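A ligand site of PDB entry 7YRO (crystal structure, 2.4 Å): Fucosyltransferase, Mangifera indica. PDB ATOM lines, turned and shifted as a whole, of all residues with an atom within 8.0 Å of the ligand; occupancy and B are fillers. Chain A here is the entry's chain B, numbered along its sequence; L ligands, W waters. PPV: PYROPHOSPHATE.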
ATOM      1  N   GLU A 177      17.972 -35.443  -7.926  1.00  0.00           N
ATOM      2  CA  GLU A 177      18.975 -35.564  -8.970  1.00  0.00           C
ATOM      3  C   GLU A 177      18.553 -36.655  -9.951  1.00  0.00           C
ATOM      4  O   GLU A 177      17.818 -37.579  -9.609  1.00  0.00           O
ATOM      5  CB  GLU A 177      20.348 -35.861  -8.379  1.00  0.00           C
ATOM      6  CG  GLU A 177      20.981 -34.694  -7.631  1.00  0.00           C
ATOM      7  CD  GLU A 177      21.171 -33.462  -8.517  1.00  0.00           C
ATOM      8  OE1 GLU A 177      21.919 -33.552  -9.509  1.00  0.00           O
ATOM      9  OE2 GLU A 177      20.571 -32.406  -8.220  1.00  0.00           O
ATOM     10  N   TRP A 227      23.724 -17.445 -20.584  1.00  0.00           N
ATOM     11  CA  TRP A 227      24.038 -18.806 -20.155  1.00  0.00           C
ATOM     12  C   TRP A 227      24.958 -18.761 -18.961  1.00  0.00           C
ATOM     13  O   TRP A 227      25.832 -17.898 -18.877  1.00  0.00           O
ATOM     14  CB  TRP A 227      24.685 -19.619 -21.286  1.00  0.00           C
ATOM     15  CG  TRP A 227      24.799 -21.083 -20.954  1.00  0.00           C
ATOM     16  CD1 TRP A 227      23.784 -21.938 -20.652  1.00  0.00           C
ATOM     17  CD2 TRP A 227      26.000 -21.871 -20.921  1.00  0.00           C
ATOM     18  NE1 TRP A 227      24.269 -23.203 -20.427  1.00  0.00           N
ATOM     19  CE2 TRP A 227      25.632 -23.185 -20.582  1.00  0.00           C
ATOM     20  CE3 TRP A 227      27.348 -21.584 -21.138  1.00  0.00           C
ATOM     21  CZ2 TRP A 227      26.559 -24.212 -20.455  1.00  0.00           C
ATOM     22  CZ3 TRP A 227      28.275 -22.611 -21.011  1.00  0.00           C
ATOM     23  CH2 TRP A 227      27.876 -23.905 -20.671  1.00  0.00           C
ATOM     24  N   SER A 228      24.769 -19.703 -18.049  1.00  0.00           N
ATOM     25  CA  SER A 228      25.646 -19.808 -16.885  1.00  0.00           C
ATOM     26  C   SER A 228      25.797 -21.270 -16.501  1.00  0.00           C
ATOM     27  O   SER A 228      24.794 -21.945 -16.209  1.00  0.00           O
ATOM     28  CB  SER A 228      25.111 -18.994 -15.712  1.00  0.00           C
ATOM     29  OG  SER A 228      26.023 -19.011 -14.633  1.00  0.00           O
ATOM     30  N   SER A 229      27.037 -21.749 -16.504  1.00  0.00           N
ATOM     31  CA  SER A 229      27.372 -23.089 -16.039  1.00  0.00           C
ATOM     32  C   SER A 229      28.756 -23.025 -15.420  1.00  0.00           C
ATOM     33  O   SER A 229      29.655 -22.396 -15.969  1.00  0.00           O
ATOM     34  CB  SER A 229      27.329 -24.103 -17.184  1.00  0.00           C
ATOM     35  OG  SER A 229      27.632 -25.414 -16.718  1.00  0.00           O
ATOM     36  N   SER A 230      28.916 -23.702 -14.280  1.00  0.00           N
ATOM     37  CA  SER A 230      30.181 -23.706 -13.570  1.00  0.00           C
ATOM     38  C   SER A 230      30.713 -25.100 -13.287  1.00  0.00           C
ATOM     39  O   SER A 230      31.830 -25.208 -12.751  1.00  0.00           O
ATOM     40  CB  SER A 230      30.064 -22.929 -12.257  1.00  0.00           C
ATOM     41  OG  SER A 230      29.828 -21.554 -12.518  1.00  0.00           O
ATOM     42  N   ARG A 231      29.964 -26.147 -13.591  1.00  0.00           N
ATOM     43  CA  ARG A 231      30.429 -27.526 -13.546  1.00  0.00           C
ATOM     44  C   ARG A 231      30.561 -27.976 -14.997  1.00  0.00           C
ATOM     45  O   ARG A 231      29.562 -28.310 -15.646  1.00  0.00           O
ATOM     46  CB  ARG A 231      29.484 -28.421 -12.756  1.00  0.00           C
ATOM     47  CG  ARG A 231      30.167 -29.607 -12.092  1.00  0.00           C
ATOM     48  CD  ARG A 231      29.172 -30.473 -11.347  1.00  0.00           C
ATOM     49  NE  ARG A 231      28.320 -31.232 -12.248  1.00  0.00           N
ATOM     50  CZ  ARG A 231      27.448 -32.155 -11.862  1.00  0.00           C
ATOM     51  NH1 ARG A 231      27.277 -32.449 -10.585  1.00  0.00           N
ATOM     52  NH2 ARG A 231      26.725 -32.795 -12.781  1.00  0.00           N
ATOM     53  N   CYS A 232      31.780 -27.966 -15.525  1.00  0.00           N
ATOM     54  CA  CYS A 232      32.018 -28.135 -16.951  1.00  0.00           C
ATOM     55  C   CYS A 232      31.951 -29.623 -17.304  1.00  0.00           C
ATOM     56  O   CYS A 232      32.881 -30.377 -17.046  1.00  0.00           O
ATOM     57  CB  CYS A 232      33.367 -27.542 -17.362  1.00  0.00           C
ATOM     58  SG  CYS A 232      33.613 -25.859 -16.765  1.00  0.00           S
ATOM     59  N   LEU A 233      30.829 -30.036 -17.883  1.00  0.00           N
ATOM     60  CA  LEU A 233      30.647 -31.387 -18.385  1.00  0.00           C
ATOM     61  C   LEU A 233      30.996 -31.427 -19.875  1.00  0.00           C
ATOM     62  O   LEU A 233      30.639 -30.513 -20.619  1.00  0.00           O
ATOM     63  CB  LEU A 233      29.214 -31.863 -18.156  1.00  0.00           C
ATOM     64  CG  LEU A 233      28.798 -31.793 -16.685  1.00  0.00           C
ATOM     65  CD1 LEU A 233      27.369 -32.271 -16.508  1.00  0.00           C
ATOM     66  CD2 LEU A 233      29.748 -32.584 -15.798  1.00  0.00           C
ATOM     67  N   ARG A 236      28.017 -31.256 -22.613  1.00  0.00           N
ATOM     68  CA  ARG A 236      27.341 -29.974 -22.497  1.00  0.00           C
ATOM     69  C   ARG A 236      28.235 -28.843 -22.964  1.00  0.00           C
ATOM     70  O   ARG A 236      27.779 -27.917 -23.652  1.00  0.00           O
ATOM     71  CB  ARG A 236      26.880 -29.735 -21.053  1.00  0.00           C
ATOM     72  CG  ARG A 236      26.485 -28.279 -20.757  1.00  0.00           C
ATOM     73  CD  ARG A 236      25.641 -28.154 -19.502  1.00  0.00           C
ATOM     74  NE  ARG A 236      26.407 -28.308 -18.274  1.00  0.00           N
ATOM     75  CZ  ARG A 236      25.864 -28.564 -17.081  1.00  0.00           C
ATOM     76  NH1 ARG A 236      24.564 -28.682 -16.927  1.00  0.00           N
ATOM     77  NH2 ARG A 236      26.657 -28.691 -16.023  1.00  0.00           N
ATOM     78  N   ASN A 237      29.524 -28.874 -22.599  1.00  0.00           N
ATOM     79  CA  ASN A 237      30.438 -27.822 -23.027  1.00  0.00           C
ATOM     80  C   ASN A 237      30.647 -27.833 -24.537  1.00  0.00           C
ATOM     81  O   ASN A 237      30.742 -26.765 -25.156  1.00  0.00           O
ATOM     82  CB  ASN A 237      31.770 -27.976 -22.294  1.00  0.00           C
ATOM     83  CG  ASN A 237      31.817 -27.159 -21.009  1.00  0.00           C
ATOM     84  OD1 ASN A 237      30.784 -26.739 -20.488  1.00  0.00           O
ATOM     85  ND2 ASN A 237      33.019 -26.947 -20.486  1.00  0.00           N
ATOM     86  N   GLY A 253      29.327 -18.238 -16.084  1.00  0.00           N
ATOM     87  CA  GLY A 253      29.882 -19.270 -15.231  1.00  0.00           C
ATOM     88  C   GLY A 253      31.356 -19.523 -15.474  1.00  0.00           C
ATOM     89  O   GLY A 253      32.022 -18.849 -16.266  1.00  0.00           O
ATOM     90  N   LYS A 254      31.879 -20.519 -14.765  1.00  0.00           N
ATOM     91  CA  LYS A 254      33.280 -20.891 -14.934  1.00  0.00           C
ATOM     92  C   LYS A 254      33.531 -21.559 -16.283  1.00  0.00           C
ATOM     93  O   LYS A 254      34.660 -21.538 -16.786  1.00  0.00           O
ATOM     94  CB  LYS A 254      33.720 -21.797 -13.783  1.00  0.00           C
ATOM     95  CG  LYS A 254      33.343 -21.249 -12.424  1.00  0.00           C
ATOM     96  CD  LYS A 254      33.795 -22.145 -11.281  1.00  0.00           C
ATOM     97  CE  LYS A 254      35.030 -21.580 -10.590  1.00  0.00           C
ATOM     98  NZ  LYS A 254      35.267 -22.233  -9.283  1.00  0.00           N
ATOM     99  N   CYS A 255      32.504 -22.172 -16.863  1.00  0.00           N
ATOM    100  CA  CYS A 255      32.621 -22.858 -18.146  1.00  0.00           C
ATOM    101  C   CYS A 255      32.353 -21.892 -19.281  1.00  0.00           C
ATOM    102  O   CYS A 255      31.314 -21.223 -19.297  1.00  0.00           O
ATOM    103  CB  CYS A 255      31.647 -24.040 -18.200  1.00  0.00           C
ATOM    104  SG  CYS A 255      31.728 -25.080 -16.732  1.00  0.00           S
ATOM    105  N   TRP A 282      24.769 -16.225  -4.120  1.00  0.00           N
ATOM    106  CA  TRP A 282      24.969 -16.394  -5.557  1.00  0.00           C
ATOM    107  C   TRP A 282      23.653 -16.411  -6.344  1.00  0.00           C
ATOM    108  O   TRP A 282      23.655 -16.086  -7.535  1.00  0.00           O
ATOM    109  CB  TRP A 282      25.756 -17.680  -5.848  1.00  0.00           C
ATOM    110  CG  TRP A 282      25.051 -18.973  -5.491  1.00  0.00           C
ATOM    111  CD1 TRP A 282      25.112 -19.639  -4.296  1.00  0.00           C
ATOM    112  CD2 TRP A 282      24.170 -19.751  -6.327  1.00  0.00           C
ATOM    113  NE1 TRP A 282      24.341 -20.780  -4.335  1.00  0.00           N
ATOM    114  CE2 TRP A 282      23.755 -20.866  -5.569  1.00  0.00           C
ATOM    115  CE3 TRP A 282      23.707 -19.609  -7.635  1.00  0.00           C
ATOM    116  CZ2 TRP A 282      22.889 -21.838  -6.085  1.00  0.00           C
ATOM    117  CZ3 TRP A 282      22.838 -20.570  -8.142  1.00  0.00           C
ATOM    118  CH2 TRP A 282      22.440 -21.665  -7.370  1.00  0.00           C
ATOM    119  N   LEU A 286      19.739 -14.086 -10.273  1.00  0.00           N
ATOM    120  CA  LEU A 286      19.667 -14.812 -11.546  1.00  0.00           C
ATOM    121  C   LEU A 286      18.448 -14.390 -12.357  1.00  0.00           C
ATOM    122  O   LEU A 286      18.567 -14.094 -13.556  1.00  0.00           O
ATOM    123  CB  LEU A 286      19.688 -16.317 -11.291  1.00  0.00           C
ATOM    124  CG  LEU A 286      21.076 -16.954 -11.187  1.00  0.00           C
ATOM    125  CD1 LEU A 286      21.943 -16.311 -10.114  1.00  0.00           C
ATOM    126  CD2 LEU A 286      20.970 -18.450 -10.958  1.00  0.00           C
ATOM    127  N   ILE A 299      20.744 -26.089 -20.533  1.00  0.00           N
ATOM    128  CA  ILE A 299      21.212 -27.426 -20.872  1.00  0.00           C
ATOM    129  C   ILE A 299      21.332 -28.219 -19.585  1.00  0.00           C
ATOM    130  O   ILE A 299      22.157 -27.891 -18.725  1.00  0.00           O
ATOM    131  CB  ILE A 299      22.555 -27.390 -21.616  1.00  0.00           C
ATOM    132  CG1 ILE A 299      22.436 -26.526 -22.873  1.00  0.00           C
ATOM    133  CG2 ILE A 299      23.000 -28.797 -21.981  1.00  0.00           C
ATOM    134  CD1 ILE A 299      23.778 -26.116 -23.437  1.00  0.00           C
ATOM    135  N   GLU A 300      20.521 -29.257 -19.450  1.00  0.00           N
ATOM    136  CA  GLU A 300      20.571 -30.073 -18.245  1.00  0.00           C
ATOM    137  C   GLU A 300      21.873 -30.850 -18.163  1.00  0.00           C
ATOM    138  O   GLU A 300      22.516 -31.140 -19.181  1.00  0.00           O
ATOM    139  CB  GLU A 300      19.382 -31.043 -18.208  1.00  0.00           C
ATOM    140  CG  GLU A 300      18.030 -30.379 -18.438  1.00  0.00           C
ATOM    141  CD  GLU A 300      17.476 -29.704 -17.194  1.00  0.00           C
ATOM    142  OE1 GLU A 300      18.230 -29.493 -16.227  1.00  0.00           O
ATOM    143  OE2 GLU A 300      16.263 -29.375 -17.211  1.00  0.00           O
ATOM    144  N   ASN A 301      22.278 -31.184 -16.940  1.00  0.00           N
ATOM    145  CA  ASN A 301      23.479 -31.990 -16.760  1.00  0.00           C
ATOM    146  C   ASN A 301      23.246 -33.448 -17.150  1.00  0.00           C
ATOM    147  O   ASN A 301      24.220 -34.191 -17.307  1.00  0.00           O
ATOM    148  CB  ASN A 301      23.974 -31.909 -15.313  1.00  0.00           C
ATOM    149  CG  ASN A 301      22.922 -32.350 -14.302  1.00  0.00           C
ATOM    150  OD1 ASN A 301      22.430 -33.481 -14.335  1.00  0.00           O
ATOM    151  ND2 ASN A 301      22.592 -31.451 -13.374  1.00  0.00           N
ATOM    152  N   THR A 302      22.000 -33.853 -17.328  1.00  0.00           N
ATOM    153  CA  THR A 302      21.642 -35.211 -17.682  1.00  0.00           C
ATOM    154  C   THR A 302      20.410 -35.151 -18.582  1.00  0.00           C
ATOM    155  O   THR A 302      19.482 -34.396 -18.298  1.00  0.00           O
ATOM    156  CB  THR A 302      21.338 -36.066 -16.441  1.00  0.00           C
ATOM    157  OG1 THR A 302      22.459 -36.047 -15.553  1.00  0.00           O
ATOM    158  CG2 THR A 302      21.029 -37.504 -16.821  1.00  0.00           C
ATOM    159  N   TYR A 307      13.358 -35.201 -16.354  1.00  0.00           N
ATOM    160  CA  TYR A 307      14.334 -34.425 -15.596  1.00  0.00           C
ATOM    161  C   TYR A 307      14.389 -33.027 -16.191  1.00  0.00           C
ATOM    162  O   TYR A 307      15.213 -32.734 -17.055  1.00  0.00           O
ATOM    163  CB  TYR A 307      15.689 -35.114 -15.593  1.00  0.00           C
ATOM    164  CG  TYR A 307      16.748 -34.386 -14.800  1.00  0.00           C
ATOM    165  CD1 TYR A 307      16.657 -34.277 -13.414  1.00  0.00           C
ATOM    166  CD2 TYR A 307      17.846 -33.808 -15.426  1.00  0.00           C
ATOM    167  CE1 TYR A 307      17.619 -33.611 -12.678  1.00  0.00           C
ATOM    168  CE2 TYR A 307      18.813 -33.152 -14.709  1.00  0.00           C
ATOM    169  CZ  TYR A 307      18.694 -33.054 -13.331  1.00  0.00           C
ATOM    170  OH  TYR A 307      19.673 -32.378 -12.621  1.00  0.00           O
ATOM    171  N   THR A 309      14.802 -29.207 -14.801  1.00  0.00           N
ATOM    172  CA  THR A 309      15.190 -28.501 -13.582  1.00  0.00           C
ATOM    173  C   THR A 309      14.909 -27.004 -13.724  1.00  0.00           C
ATOM    174  O   THR A 309      14.321 -26.545 -14.710  1.00  0.00           O
ATOM    175  CB  THR A 309      16.661 -28.753 -13.265  1.00  0.00           C
ATOM    176  OG1 THR A 309      17.495 -28.072 -14.208  1.00  0.00           O
ATOM    177  CG2 THR A 309      16.970 -30.234 -13.294  1.00  0.00           C
ATOM    178  N   GLU A 310      15.338 -26.233 -12.724  1.00  0.00           N
ATOM    179  CA  GLU A 310      15.106 -24.802 -12.673  1.00  0.00           C
ATOM    180  C   GLU A 310      15.811 -24.034 -13.789  1.00  0.00           C
ATOM    181  O   GLU A 310      15.498 -22.858 -13.995  1.00  0.00           O
ATOM    182  CB  GLU A 310      15.533 -24.233 -11.328  1.00  0.00           C
ATOM    183  CG  GLU A 310      17.037 -24.049 -11.176  1.00  0.00           C
ATOM    184  CD  GLU A 310      17.788 -25.356 -11.083  1.00  0.00           C
ATOM    185  OE1 GLU A 310      17.186 -26.379 -10.692  1.00  0.00           O
ATOM    186  OE2 GLU A 310      18.992 -25.372 -11.408  1.00  0.00           O
ATOM    187  N   LYS A 311      16.756 -24.668 -14.507  1.00  0.00           N
ATOM    188  CA  LYS A 311      17.420 -24.000 -15.622  1.00  0.00           C
ATOM    189  C   LYS A 311      16.409 -23.502 -16.655  1.00  0.00           C
ATOM    190  O   LYS A 311      16.663 -22.496 -17.321  1.00  0.00           O
ATOM    191  CB  LYS A 311      18.428 -24.953 -16.263  1.00  0.00           C
ATOM    192  CG  LYS A 311      19.536 -25.412 -15.317  1.00  0.00           C
ATOM    193  CD  LYS A 311      20.522 -26.336 -16.028  1.00  0.00           C
ATOM    194  CE  LYS A 311      21.694 -26.707 -15.128  1.00  0.00           C
ATOM    195  NZ  LYS A 311      21.267 -27.422 -13.893  1.00  0.00           N
HETATM  196  O11 PPV L   1      27.256 -26.206 -13.420  1.00  0.00           O
HETATM  197  P1  PPV L   1      25.857 -25.733 -13.701  1.00  0.00           P
HETATM  198  O21 PPV L   1      25.523 -25.944 -15.163  1.00  0.00           O
HETATM  199  O31 PPV L   1      25.757 -24.256 -13.385  1.00  0.00           O
HETATM  200  OPP PPV L   1      24.774 -26.555 -12.753  1.00  0.00           O
HETATM  201  P2  PPV L   1      24.849 -28.167 -12.356  1.00  0.00           P
HETATM  202  O12 PPV L   1      26.197 -28.473 -11.750  1.00  0.00           O
HETATM  203  O22 PPV L   1      23.772 -28.467 -11.334  1.00  0.00           O
HETATM  204  O32 PPV L   1      24.643 -29.013 -13.592  1.00  0.00           O
HETATM  205  O   HOH W   1      25.377 -30.206  -9.910  1.00  0.00           O
HETATM  206  O   HOH W   2      26.094 -22.033 -11.318  1.00  0.00           O
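O of Ser 229 lies within hydrogen-bond range of N of Cys 255, at 3.0 Å.
The side-chain hydroxyl (OG) of Ser 230 lies within hydrogen-bond range of the backbone NH (N) of Lys 254 (3.2 Å).
The side-chain carboxylate (OE2) of Glu 310 lies within salt-bridge range of the side-chain amino group (NZ) of Lys 311.
O of Ile 299 lies within hydrogen-bond range of NH1 of Arg 236 (3.1 Å).
The side-chain sulfur (SG) of Cys 232 is disulfide-bonded to the side-chain sulfur (SG) of Cys 255, 2.0 Å away.
The side-chain hydroxyl of Ser 229 is in hydrogen-bond range of the guanidinium group of Arg 236.
The side-chain hydroxyl (OG1) of Thr 302 sits at hydrogen-bond distance from the side-chain amide oxygen (OD1) of Asn 301 (2.8 Å).
N of Lys 311 sits close to OG1 of Thr 309 (3.5 Å).
Water W1 lies within hydrogen-bond range of O12 of the ligand (2.7 Å) and NH1 of Arg 231 (3.0 Å).
Merely in contact with the ligand: Ser 228 (3.8 Å).
Seven residues have an atom within 4 Å of the ligand: Ser 228, Ser 229, Ser 230, Arg 231, Arg 236, Asn 301 and Lys 311.
The side-chain amino group (NZ) of Lys 311 lies within salt-bridge range of an oxygen (O22) of the ligand, at 3.7 Å.
NE of Arg 231 is in salt-bridge range of O12 of the ligand.
The guanidinium group (NH2) of Arg 236 lies within salt-bridge range of an oxygen (O21) of the ligand (3.1 Å).
The backbone NH (N) of Ser 230 is in hydrogen-bond range of an oxygen (O11) of the ligand.
The backbone NH of Arg 231 sits at hydrogen-bond distance from an oxygen (O11) of the ligand (2.7 Å).
The side-chain hydroxyl (OG) of Ser 229 sits at hydrogen-bond distance from an oxygen (O21) of the ligand (2.7 Å).
The side-chain amide nitrogen (ND2) of Asn 301 is in hydrogen-bond range of an oxygen (O32) of the ligand.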
